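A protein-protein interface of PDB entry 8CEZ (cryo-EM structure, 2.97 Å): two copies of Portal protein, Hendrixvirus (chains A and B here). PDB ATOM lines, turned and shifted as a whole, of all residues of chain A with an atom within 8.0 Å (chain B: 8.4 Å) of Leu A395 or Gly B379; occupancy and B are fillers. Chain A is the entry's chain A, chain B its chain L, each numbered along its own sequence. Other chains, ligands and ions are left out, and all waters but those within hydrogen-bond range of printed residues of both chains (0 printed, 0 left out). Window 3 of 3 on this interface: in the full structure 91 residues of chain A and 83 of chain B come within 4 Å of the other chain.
Of the 15 printed residues of chain B, 7 touch a printed residue of chain A. Hydrophobic or aromatic side chains of chain A that line the printed part of chain B: Ile A383, Met A386, Met A392 and Leu A395. Among the printed residues, 11 pairs touch across the chains. Among the printed residues, Asp or Glu carboxylates within 4 Å of a Lys or Arg side-chain nitrogen of the other chain: Lys A373 with Glu B377 (3.4 Å) and Arg A387 with Glu B385 (3.1 Å).
CG2 of Ile A383 touches O of Gly B379, at 3.5 Å. Ile A383 touches Leu B380. Leu B380 touches Met A386. CD1 of Leu A395 touches O of Gly B379, 3.7 Å away.
O of Ala B374 lies within hydrogen-bond range of NZ of Lys A373 (3.4 Å). The side-chain amino group of Lys A373 is in salt-bridge range of the side-chain carboxylate of Glu B377 (3.4 Å). The side-chain amino group of Lys A373 is in hydrogen-bond range of the side-chain hydroxyl of Ser B378, 2.6 Å away. The guanidinium group (NH1) of Arg A387 is in hydrogen-bond range of the backbone carbonyl oxygen (O) of Leu B380, 3.0 Å away. OE1 of Glu B385 is in salt-bridge range of NH1 of Arg A387 (3.1 Å). The guanidinium group (NE) of Arg B381 sits close to the side-chain sulfur (SD) of Met A392, at 3.7 Å. SD of Met A392 lies close to OE1 of Glu B385, 3.1 Å away.
Positions printed for both chains: 373, 383, 385, 386 and 398. Of the 11 pairs that touch across the chains among the printed residues, none has its exchanged pair printed and touching as well.
Of chain B, only Gly B379 comes within 4 Å of Leu A395. Gly B379 touches just these residues of chain A: Ile A383 and Leu A395. No residue of chain B comes within 4 Å of Pro A396. Printed residues of chain A within 4 Å of Leu B380: Ile A383 (3.7 Å), Met A386 (3.7 Å) and Arg A387 (3.0 Å). Of the printed residues of chain A, Glu B385 touches Arg A387 and Met A392. Printed residues of chain A within 4 Å of Arg B381: Met A392 (3.3 Å). Of the printed residues of chain A, Ser B378 touches Lys A373. Of the printed residues of chain A, Glu B377 touches Lys A373 (3.2 Å). Met B386 touches none of the printed residues of chain A. Lys B373 touches none of the printed residues of chain A. The nearest residue of chain A that does not touch Gly B379 is Arg A387 (5.1 Å). The nearest printed residue of chain B that does not touch Met A386 is Arg B381 (5.6 Å).
OD1 of Asn A384 sits at hydrogen-bond distance from N of Leu A395 (2.9 Å). The guanidinium group of Arg A387 is in hydrogen-bond range of the side-chain sulfur of Met A392, at 2.9 Å. NH2 of Arg A387 sits at hydrogen-bond distance from O of Pro A393 (2.7 Å). The backbone carbonyl oxygen (O) of Ala B374 lies within hydrogen-bond range of the side-chain hydroxyl (OG) of Ser B378. The backbone carbonyl oxygen (O) of Met B375 is in hydrogen-bond range of the backbone NH (N) of Arg B381 (3.1 Å). The backbone NH of Glu B385 lies close to the side-chain hydroxyl of Thr B382.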
ATOM      1  N   LYS A 373      -9.107 -17.769  -8.155  1.00  0.00           N
ATOM      2  CA  LYS A 373      -9.036 -18.585  -9.362  1.00  0.00           C
ATOM      3  C   LYS A 373      -7.650 -18.516  -9.990  1.00  0.00           C
ATOM      4  O   LYS A 373      -7.077 -19.546 -10.367  1.00  0.00           O
ATOM      5  CB  LYS A 373     -10.096 -18.126 -10.361  1.00  0.00           C
ATOM      6  CG  LYS A 373     -10.138 -18.953 -11.635  1.00  0.00           C
ATOM      7  CD  LYS A 373     -11.458 -18.818 -12.388  1.00  0.00           C
ATOM      8  CE  LYS A 373     -12.645 -19.375 -11.608  1.00  0.00           C
ATOM      9  NZ  LYS A 373     -12.479 -20.810 -11.249  1.00  0.00           N
ATOM     10  N   ILE A 383      -6.085 -25.562  -2.320  1.00  0.00           N
ATOM     11  CA  ILE A 383      -7.487 -25.283  -2.027  1.00  0.00           C
ATOM     12  C   ILE A 383      -7.671 -24.973  -0.547  1.00  0.00           C
ATOM     13  O   ILE A 383      -8.428 -24.071  -0.177  1.00  0.00           O
ATOM     14  CB  ILE A 383      -8.368 -26.464  -2.473  1.00  0.00           C
ATOM     15  CG1 ILE A 383      -8.412 -26.537  -4.000  1.00  0.00           C
ATOM     16  CG2 ILE A 383      -9.764 -26.336  -1.895  1.00  0.00           C
ATOM     17  CD1 ILE A 383      -8.935 -27.841  -4.542  1.00  0.00           C
ATOM     18  N   ASN A 384      -6.986 -25.718   0.320  1.00  0.00           N
ATOM     19  CA  ASN A 384      -7.160 -25.528   1.756  1.00  0.00           C
ATOM     20  C   ASN A 384      -6.569 -24.205   2.218  1.00  0.00           C
ATOM     21  O   ASN A 384      -7.099 -23.571   3.135  1.00  0.00           O
ATOM     22  CB  ASN A 384      -6.526 -26.689   2.514  1.00  0.00           C
ATOM     23  CG  ASN A 384      -7.347 -27.952   2.426  1.00  0.00           C
ATOM     24  OD1 ASN A 384      -8.533 -27.912   2.117  1.00  0.00           O
ATOM     25  ND2 ASN A 384      -6.719 -29.082   2.708  1.00  0.00           N
ATOM     26  N   GLU A 385      -5.471 -23.770   1.601  1.00  0.00           N
ATOM     27  CA  GLU A 385      -4.883 -22.489   1.973  1.00  0.00           C
ATOM     28  C   GLU A 385      -5.847 -21.343   1.697  1.00  0.00           C
ATOM     29  O   GLU A 385      -5.969 -20.418   2.508  1.00  0.00           O
ATOM     30  CB  GLU A 385      -3.574 -22.280   1.217  1.00  0.00           C
ATOM     31  CG  GLU A 385      -2.411 -23.037   1.808  1.00  0.00           C
ATOM     32  CD  GLU A 385      -1.157 -22.909   0.979  1.00  0.00           C
ATOM     33  OE1 GLU A 385      -1.126 -22.043   0.080  1.00  0.00           O
ATOM     34  OE2 GLU A 385      -0.207 -23.677   1.225  1.00  0.00           O
ATOM     35  N   MET A 386      -6.536 -21.385   0.556  1.00  0.00           N
ATOM     36  CA  MET A 386      -7.513 -20.351   0.236  1.00  0.00           C
ATOM     37  C   MET A 386      -8.804 -20.521   1.024  1.00  0.00           C
ATOM     38  O   MET A 386      -9.502 -19.534   1.279  1.00  0.00           O
ATOM     39  CB  MET A 386      -7.812 -20.364  -1.261  1.00  0.00           C
ATOM     40  CG  MET A 386      -6.827 -19.564  -2.094  1.00  0.00           C
ATOM     41  SD  MET A 386      -6.953 -19.907  -3.856  1.00  0.00           S
ATOM     42  CE  MET A 386      -6.593 -21.659  -3.906  1.00  0.00           C
ATOM     43  N   ARG A 387      -9.148 -21.756   1.396  1.00  0.00           N
ATOM     44  CA  ARG A 387     -10.317 -21.978   2.240  1.00  0.00           C
ATOM     45  C   ARG A 387     -10.090 -21.425   3.640  1.00  0.00           C
ATOM     46  O   ARG A 387     -11.021 -20.918   4.273  1.00  0.00           O
ATOM     47  CB  ARG A 387     -10.643 -23.470   2.297  1.00  0.00           C
ATOM     48  CG  ARG A 387     -11.640 -23.929   1.254  1.00  0.00           C
ATOM     49  CD  ARG A 387     -11.714 -25.439   1.174  1.00  0.00           C
ATOM     50  NE  ARG A 387     -12.567 -26.024   2.202  1.00  0.00           N
ATOM     51  CZ  ARG A 387     -13.892 -25.959   2.206  1.00  0.00           C
ATOM     52  NH1 ARG A 387     -14.555 -25.302   1.271  1.00  0.00           N
ATOM     53  NH2 ARG A 387     -14.566 -26.569   3.173  1.00  0.00           N
ATOM     54  N   MET A 392     -12.957 -21.648   6.742  1.00  0.00           N
ATOM     55  CA  MET A 392     -13.792 -22.786   6.405  1.00  0.00           C
ATOM     56  C   MET A 392     -12.956 -24.053   6.519  1.00  0.00           C
ATOM     57  O   MET A 392     -11.750 -24.021   6.258  1.00  0.00           O
ATOM     58  CB  MET A 392     -14.348 -22.603   4.988  1.00  0.00           C
ATOM     59  CG  MET A 392     -15.340 -23.634   4.522  1.00  0.00           C
ATOM     60  SD  MET A 392     -15.914 -23.257   2.863  1.00  0.00           S
ATOM     61  CE  MET A 392     -16.934 -21.830   3.245  1.00  0.00           C
ATOM     62  N   PRO A 393     -13.556 -25.179   6.922  1.00  0.00           N
ATOM     63  CA  PRO A 393     -12.742 -26.328   7.312  1.00  0.00           C
ATOM     64  C   PRO A 393     -12.054 -26.950   6.111  1.00  0.00           C
ATOM     65  O   PRO A 393     -12.533 -26.824   4.972  1.00  0.00           O
ATOM     66  CB  PRO A 393     -13.764 -27.294   7.939  1.00  0.00           C
ATOM     67  CG  PRO A 393     -15.047 -26.577   7.990  1.00  0.00           C
ATOM     68  CD  PRO A 393     -14.991 -25.495   6.989  1.00  0.00           C
ATOM     69  N   PRO A 394     -10.934 -27.642   6.316  1.00  0.00           N
ATOM     70  CA  PRO A 394     -10.210 -28.224   5.180  1.00  0.00           C
ATOM     71  C   PRO A 394     -11.036 -29.263   4.438  1.00  0.00           C
ATOM     72  O   PRO A 394     -11.916 -29.915   5.005  1.00  0.00           O
ATOM     73  CB  PRO A 394      -8.979 -28.863   5.830  1.00  0.00           C
ATOM     74  CG  PRO A 394      -8.849 -28.220   7.146  1.00  0.00           C
ATOM     75  CD  PRO A 394     -10.231 -27.879   7.586  1.00  0.00           C
ATOM     76  N   LEU A 395     -10.743 -29.406   3.145  1.00  0.00           N
ATOM     77  CA  LEU A 395     -11.355 -30.425   2.316  1.00  0.00           C
ATOM     78  C   LEU A 395     -10.369 -31.562   2.060  1.00  0.00           C
ATOM     79  O   LEU A 395      -9.153 -31.353   2.096  1.00  0.00           O
ATOM     80  CB  LEU A 395     -11.818 -29.855   0.970  1.00  0.00           C
ATOM     81  CG  LEU A 395     -13.192 -29.186   0.956  1.00  0.00           C
ATOM     82  CD1 LEU A 395     -13.466 -28.539  -0.391  1.00  0.00           C
ATOM     83  CD2 LEU A 395     -14.286 -30.174   1.303  1.00  0.00           C
ATOM     84  N   PRO A 396     -10.858 -32.781   1.809  1.00  0.00           N
ATOM     85  CA  PRO A 396      -9.950 -33.888   1.475  1.00  0.00           C
ATOM     86  C   PRO A 396      -9.354 -33.793   0.076  1.00  0.00           C
ATOM     87  O   PRO A 396      -9.901 -34.344  -0.883  1.00  0.00           O
ATOM     88  CB  PRO A 396     -10.843 -35.126   1.620  1.00  0.00           C
ATOM     89  CG  PRO A 396     -11.913 -34.715   2.542  1.00  0.00           C
ATOM     90  CD  PRO A 396     -12.173 -33.278   2.248  1.00  0.00           C
ATOM     91  N   GLY A 397      -8.216 -33.113  -0.044  1.00  0.00           N
ATOM     92  CA  GLY A 397      -7.577 -32.911  -1.328  1.00  0.00           C
ATOM     93  C   GLY A 397      -7.187 -31.470  -1.592  1.00  0.00           C
ATOM     94  O   GLY A 397      -6.957 -31.088  -2.741  1.00  0.00           O
ATOM     95  N   GLY A 398      -7.099 -30.665  -0.539  1.00  0.00           N
ATOM     96  CA  GLY A 398      -6.673 -29.283  -0.668  1.00  0.00           C
ATOM     97  C   GLY A 398      -5.329 -29.009  -0.022  1.00  0.00           C
ATOM     98  O   GLY A 398      -4.290 -29.474  -0.489  1.00  0.00           O
ATOM     99  N   MET B 372     -20.312 -17.731  -7.048  1.00  0.00           N
ATOM    100  CA  MET B 372     -20.544 -19.150  -6.799  1.00  0.00           C
ATOM    101  C   MET B 372     -19.988 -20.009  -7.927  1.00  0.00           C
ATOM    102  O   MET B 372     -19.441 -21.086  -7.674  1.00  0.00           O
ATOM    103  CB  MET B 372     -22.035 -19.425  -6.599  1.00  0.00           C
ATOM    104  CG  MET B 372     -22.653 -18.655  -5.445  1.00  0.00           C
ATOM    105  SD  MET B 372     -24.140 -19.434  -4.794  1.00  0.00           S
ATOM    106  CE  MET B 372     -25.276 -18.050  -4.805  1.00  0.00           C
ATOM    107  N   LYS B 373     -20.114 -19.558  -9.175  1.00  0.00           N
ATOM    108  CA  LYS B 373     -19.526 -20.298 -10.286  1.00  0.00           C
ATOM    109  C   LYS B 373     -18.016 -20.406 -10.129  1.00  0.00           C
ATOM    110  O   LYS B 373     -17.435 -21.481 -10.329  1.00  0.00           O
ATOM    111  CB  LYS B 373     -19.879 -19.612 -11.605  1.00  0.00           C
ATOM    112  CG  LYS B 373     -19.363 -20.340 -12.837  1.00  0.00           C
ATOM    113  CD  LYS B 373     -20.123 -19.974 -14.105  1.00  0.00           C
ATOM    114  CE  LYS B 373     -21.583 -20.404 -14.064  1.00  0.00           C
ATOM    115  NZ  LYS B 373     -21.747 -21.854 -13.778  1.00  0.00           N
ATOM    116  N   ALA B 374     -17.364 -19.301  -9.763  1.00  0.00           N
ATOM    117  CA  ALA B 374     -15.919 -19.326  -9.569  1.00  0.00           C
ATOM    118  C   ALA B 374     -15.527 -20.256  -8.426  1.00  0.00           C
ATOM    119  O   ALA B 374     -14.573 -21.032  -8.548  1.00  0.00           O
ATOM    120  CB  ALA B 374     -15.405 -17.913  -9.312  1.00  0.00           C
ATOM    121  N   MET B 375     -16.253 -20.195  -7.308  1.00  0.00           N
ATOM    122  CA  MET B 375     -15.916 -21.035  -6.162  1.00  0.00           C
ATOM    123  C   MET B 375     -16.261 -22.498  -6.418  1.00  0.00           C
ATOM    124  O   MET B 375     -15.738 -23.390  -5.742  1.00  0.00           O
ATOM    125  CB  MET B 375     -16.644 -20.536  -4.914  1.00  0.00           C
ATOM    126  CG  MET B 375     -16.265 -19.132  -4.446  1.00  0.00           C
ATOM    127  SD  MET B 375     -14.520 -18.902  -4.053  1.00  0.00           S
ATOM    128  CE  MET B 375     -13.874 -18.356  -5.630  1.00  0.00           C
ATOM    129  N   GLY B 376     -17.143 -22.766  -7.379  1.00  0.00           N
ATOM    130  CA  GLY B 376     -17.541 -24.138  -7.637  1.00  0.00           C
ATOM    131  C   GLY B 376     -16.666 -24.827  -8.664  1.00  0.00           C
ATOM    132  O   GLY B 376     -16.353 -26.012  -8.527  1.00  0.00           O
ATOM    133  N   GLU B 377     -16.260 -24.104  -9.707  1.00  0.00           N
ATOM    134  CA  GLU B 377     -15.413 -24.707 -10.728  1.00  0.00           C
ATOM    135  C   GLU B 377     -13.943 -24.718 -10.337  1.00  0.00           C
ATOM    136  O   GLU B 377     -13.114 -25.196 -11.117  1.00  0.00           O
ATOM    137  CB  GLU B 377     -15.601 -23.984 -12.063  1.00  0.00           C
ATOM    138  CG  GLU B 377     -14.956 -22.613 -12.149  1.00  0.00           C
ATOM    139  CD  GLU B 377     -15.616 -21.725 -13.190  1.00  0.00           C
ATOM    140  OE1 GLU B 377     -16.615 -22.157 -13.801  1.00  0.00           O
ATOM    141  OE2 GLU B 377     -15.131 -20.595 -13.405  1.00  0.00           O
ATOM    142  N   SER B 378     -13.607 -24.211  -9.154  1.00  0.00           N
ATOM    143  CA  SER B 378     -12.251 -24.256  -8.631  1.00  0.00           C
ATOM    144  C   SER B 378     -12.048 -25.353  -7.597  1.00  0.00           C
ATOM    145  O   SER B 378     -10.899 -25.688  -7.293  1.00  0.00           O
ATOM    146  CB  SER B 378     -11.892 -22.909  -8.003  1.00  0.00           C
ATOM    147  OG  SER B 378     -11.846 -21.891  -8.981  1.00  0.00           O
ATOM    148  N   GLY B 379     -13.125 -25.924  -7.063  1.00  0.00           N
ATOM    149  CA  GLY B 379     -13.022 -26.855  -5.962  1.00  0.00           C
ATOM    150  C   GLY B 379     -12.970 -26.208  -4.599  1.00  0.00           C
ATOM    151  O   GLY B 379     -12.784 -26.914  -3.603  1.00  0.00           O
ATOM    152  N   LEU B 380     -13.132 -24.887  -4.521  1.00  0.00           N
ATOM    153  CA  LEU B 380     -13.066 -24.168  -3.257  1.00  0.00           C
ATOM    154  C   LEU B 380     -14.351 -24.265  -2.450  1.00  0.00           C
ATOM    155  O   LEU B 380     -14.363 -23.848  -1.289  1.00  0.00           O
ATOM    156  CB  LEU B 380     -12.747 -22.694  -3.512  1.00  0.00           C
ATOM    157  CG  LEU B 380     -11.362 -22.374  -4.070  1.00  0.00           C
ATOM    158  CD1 LEU B 380     -11.343 -20.970  -4.648  1.00  0.00           C
ATOM    159  CD2 LEU B 380     -10.299 -22.535  -3.002  1.00  0.00           C
ATOM    160  N   ARG B 381     -15.429 -24.778  -3.034  1.00  0.00           N
ATOM    161  CA  ARG B 381     -16.696 -24.933  -2.338  1.00  0.00           C
ATOM    162  C   ARG B 381     -17.406 -26.168  -2.864  1.00  0.00           C
ATOM    163  O   ARG B 381     -17.329 -26.485  -4.053  1.00  0.00           O
ATOM    164  CB  ARG B 381     -17.610 -23.716  -2.526  1.00  0.00           C
ATOM    165  CG  ARG B 381     -17.091 -22.420  -1.947  1.00  0.00           C
ATOM    166  CD  ARG B 381     -17.233 -22.373  -0.444  1.00  0.00           C
ATOM    167  NE  ARG B 381     -17.018 -21.026   0.068  1.00  0.00           N
ATOM    168  CZ  ARG B 381     -15.830 -20.456   0.216  1.00  0.00           C
ATOM    169  NH1 ARG B 381     -14.713 -21.099  -0.080  1.00  0.00           N
ATOM    170  NH2 ARG B 381     -15.763 -19.212   0.674  1.00  0.00           N
ATOM    171  N   THR B 382     -18.098 -26.862  -1.970  1.00  0.00           N
ATOM    172  CA  THR B 382     -19.015 -27.921  -2.360  1.00  0.00           C
ATOM    173  C   THR B 382     -20.379 -27.317  -2.670  1.00  0.00           C
ATOM    174  O   THR B 382     -20.703 -26.205  -2.250  1.00  0.00           O
ATOM    175  CB  THR B 382     -19.149 -28.978  -1.261  1.00  0.00           C
ATOM    176  OG1 THR B 382     -19.877 -28.432  -0.156  1.00  0.00           O
ATOM    177  CG2 THR B 382     -17.786 -29.440  -0.787  1.00  0.00           C
ATOM    178  N   ILE B 383     -21.179 -28.066  -3.427  1.00  0.00           N
ATOM    179  CA  ILE B 383     -22.497 -27.574  -3.813  1.00  0.00           C
ATOM    180  C   ILE B 383     -23.365 -27.362  -2.580  1.00  0.00           C
ATOM    181  O   ILE B 383     -24.098 -26.373  -2.483  1.00  0.00           O
ATOM    182  CB  ILE B 383     -23.155 -28.542  -4.813  1.00  0.00           C
ATOM    183  CG1 ILE B 383     -22.418 -28.490  -6.152  1.00  0.00           C
ATOM    184  CG2 ILE B 383     -24.621 -28.205  -4.990  1.00  0.00           C
ATOM    185  CD1 ILE B 383     -22.724 -29.645  -7.066  1.00  0.00           C
ATOM    186  N   GLU B 385     -22.343 -26.683   0.431  1.00  0.00           N
ATOM    187  CA  GLU B 385     -21.843 -25.535   1.176  1.00  0.00           C
ATOM    188  C   GLU B 385     -22.410 -24.234   0.627  1.00  0.00           C
ATOM    189  O   GLU B 385     -22.785 -23.339   1.392  1.00  0.00           O
ATOM    190  CB  GLU B 385     -20.317 -25.511   1.139  1.00  0.00           C
ATOM    191  CG  GLU B 385     -19.666 -26.436   2.145  1.00  0.00           C
ATOM    192  CD  GLU B 385     -18.157 -26.386   2.085  1.00  0.00           C
ATOM    193  OE1 GLU B 385     -17.617 -25.455   1.454  1.00  0.00           O
ATOM    194  OE2 GLU B 385     -17.509 -27.283   2.663  1.00  0.00           O
ATOM    195  N   MET B 386     -22.471 -24.102  -0.698  1.00  0.00           N
ATOM    196  CA  MET B 386     -23.031 -22.898  -1.300  1.00  0.00           C
ATOM    197  C   MET B 386     -24.553 -22.888  -1.262  1.00  0.00           C
ATOM    198  O   MET B 386     -25.161 -21.814  -1.342  1.00  0.00           O
ATOM    199  CB  MET B 386     -22.543 -22.763  -2.741  1.00  0.00           C
ATOM    200  CG  MET B 386     -21.258 -21.959  -2.880  1.00  0.00           C
ATOM    201  SD  MET B 386     -20.582 -21.936  -4.552  1.00  0.00           S
ATOM    202  CE  MET B 386     -20.537 -23.682  -4.950  1.00  0.00           C
ATOM    203  N   GLY B 398     -23.398 -32.995  -3.023  1.00  0.00           N
ATOM    204  CA  GLY B 398     -22.884 -31.656  -2.804  1.00  0.00           C
ATOM    205  C   GLY B 398     -21.881 -31.578  -1.672  1.00  0.00           C
ATOM    206  O   GLY B 398     -21.160 -32.535  -1.393  1.00  0.00           O
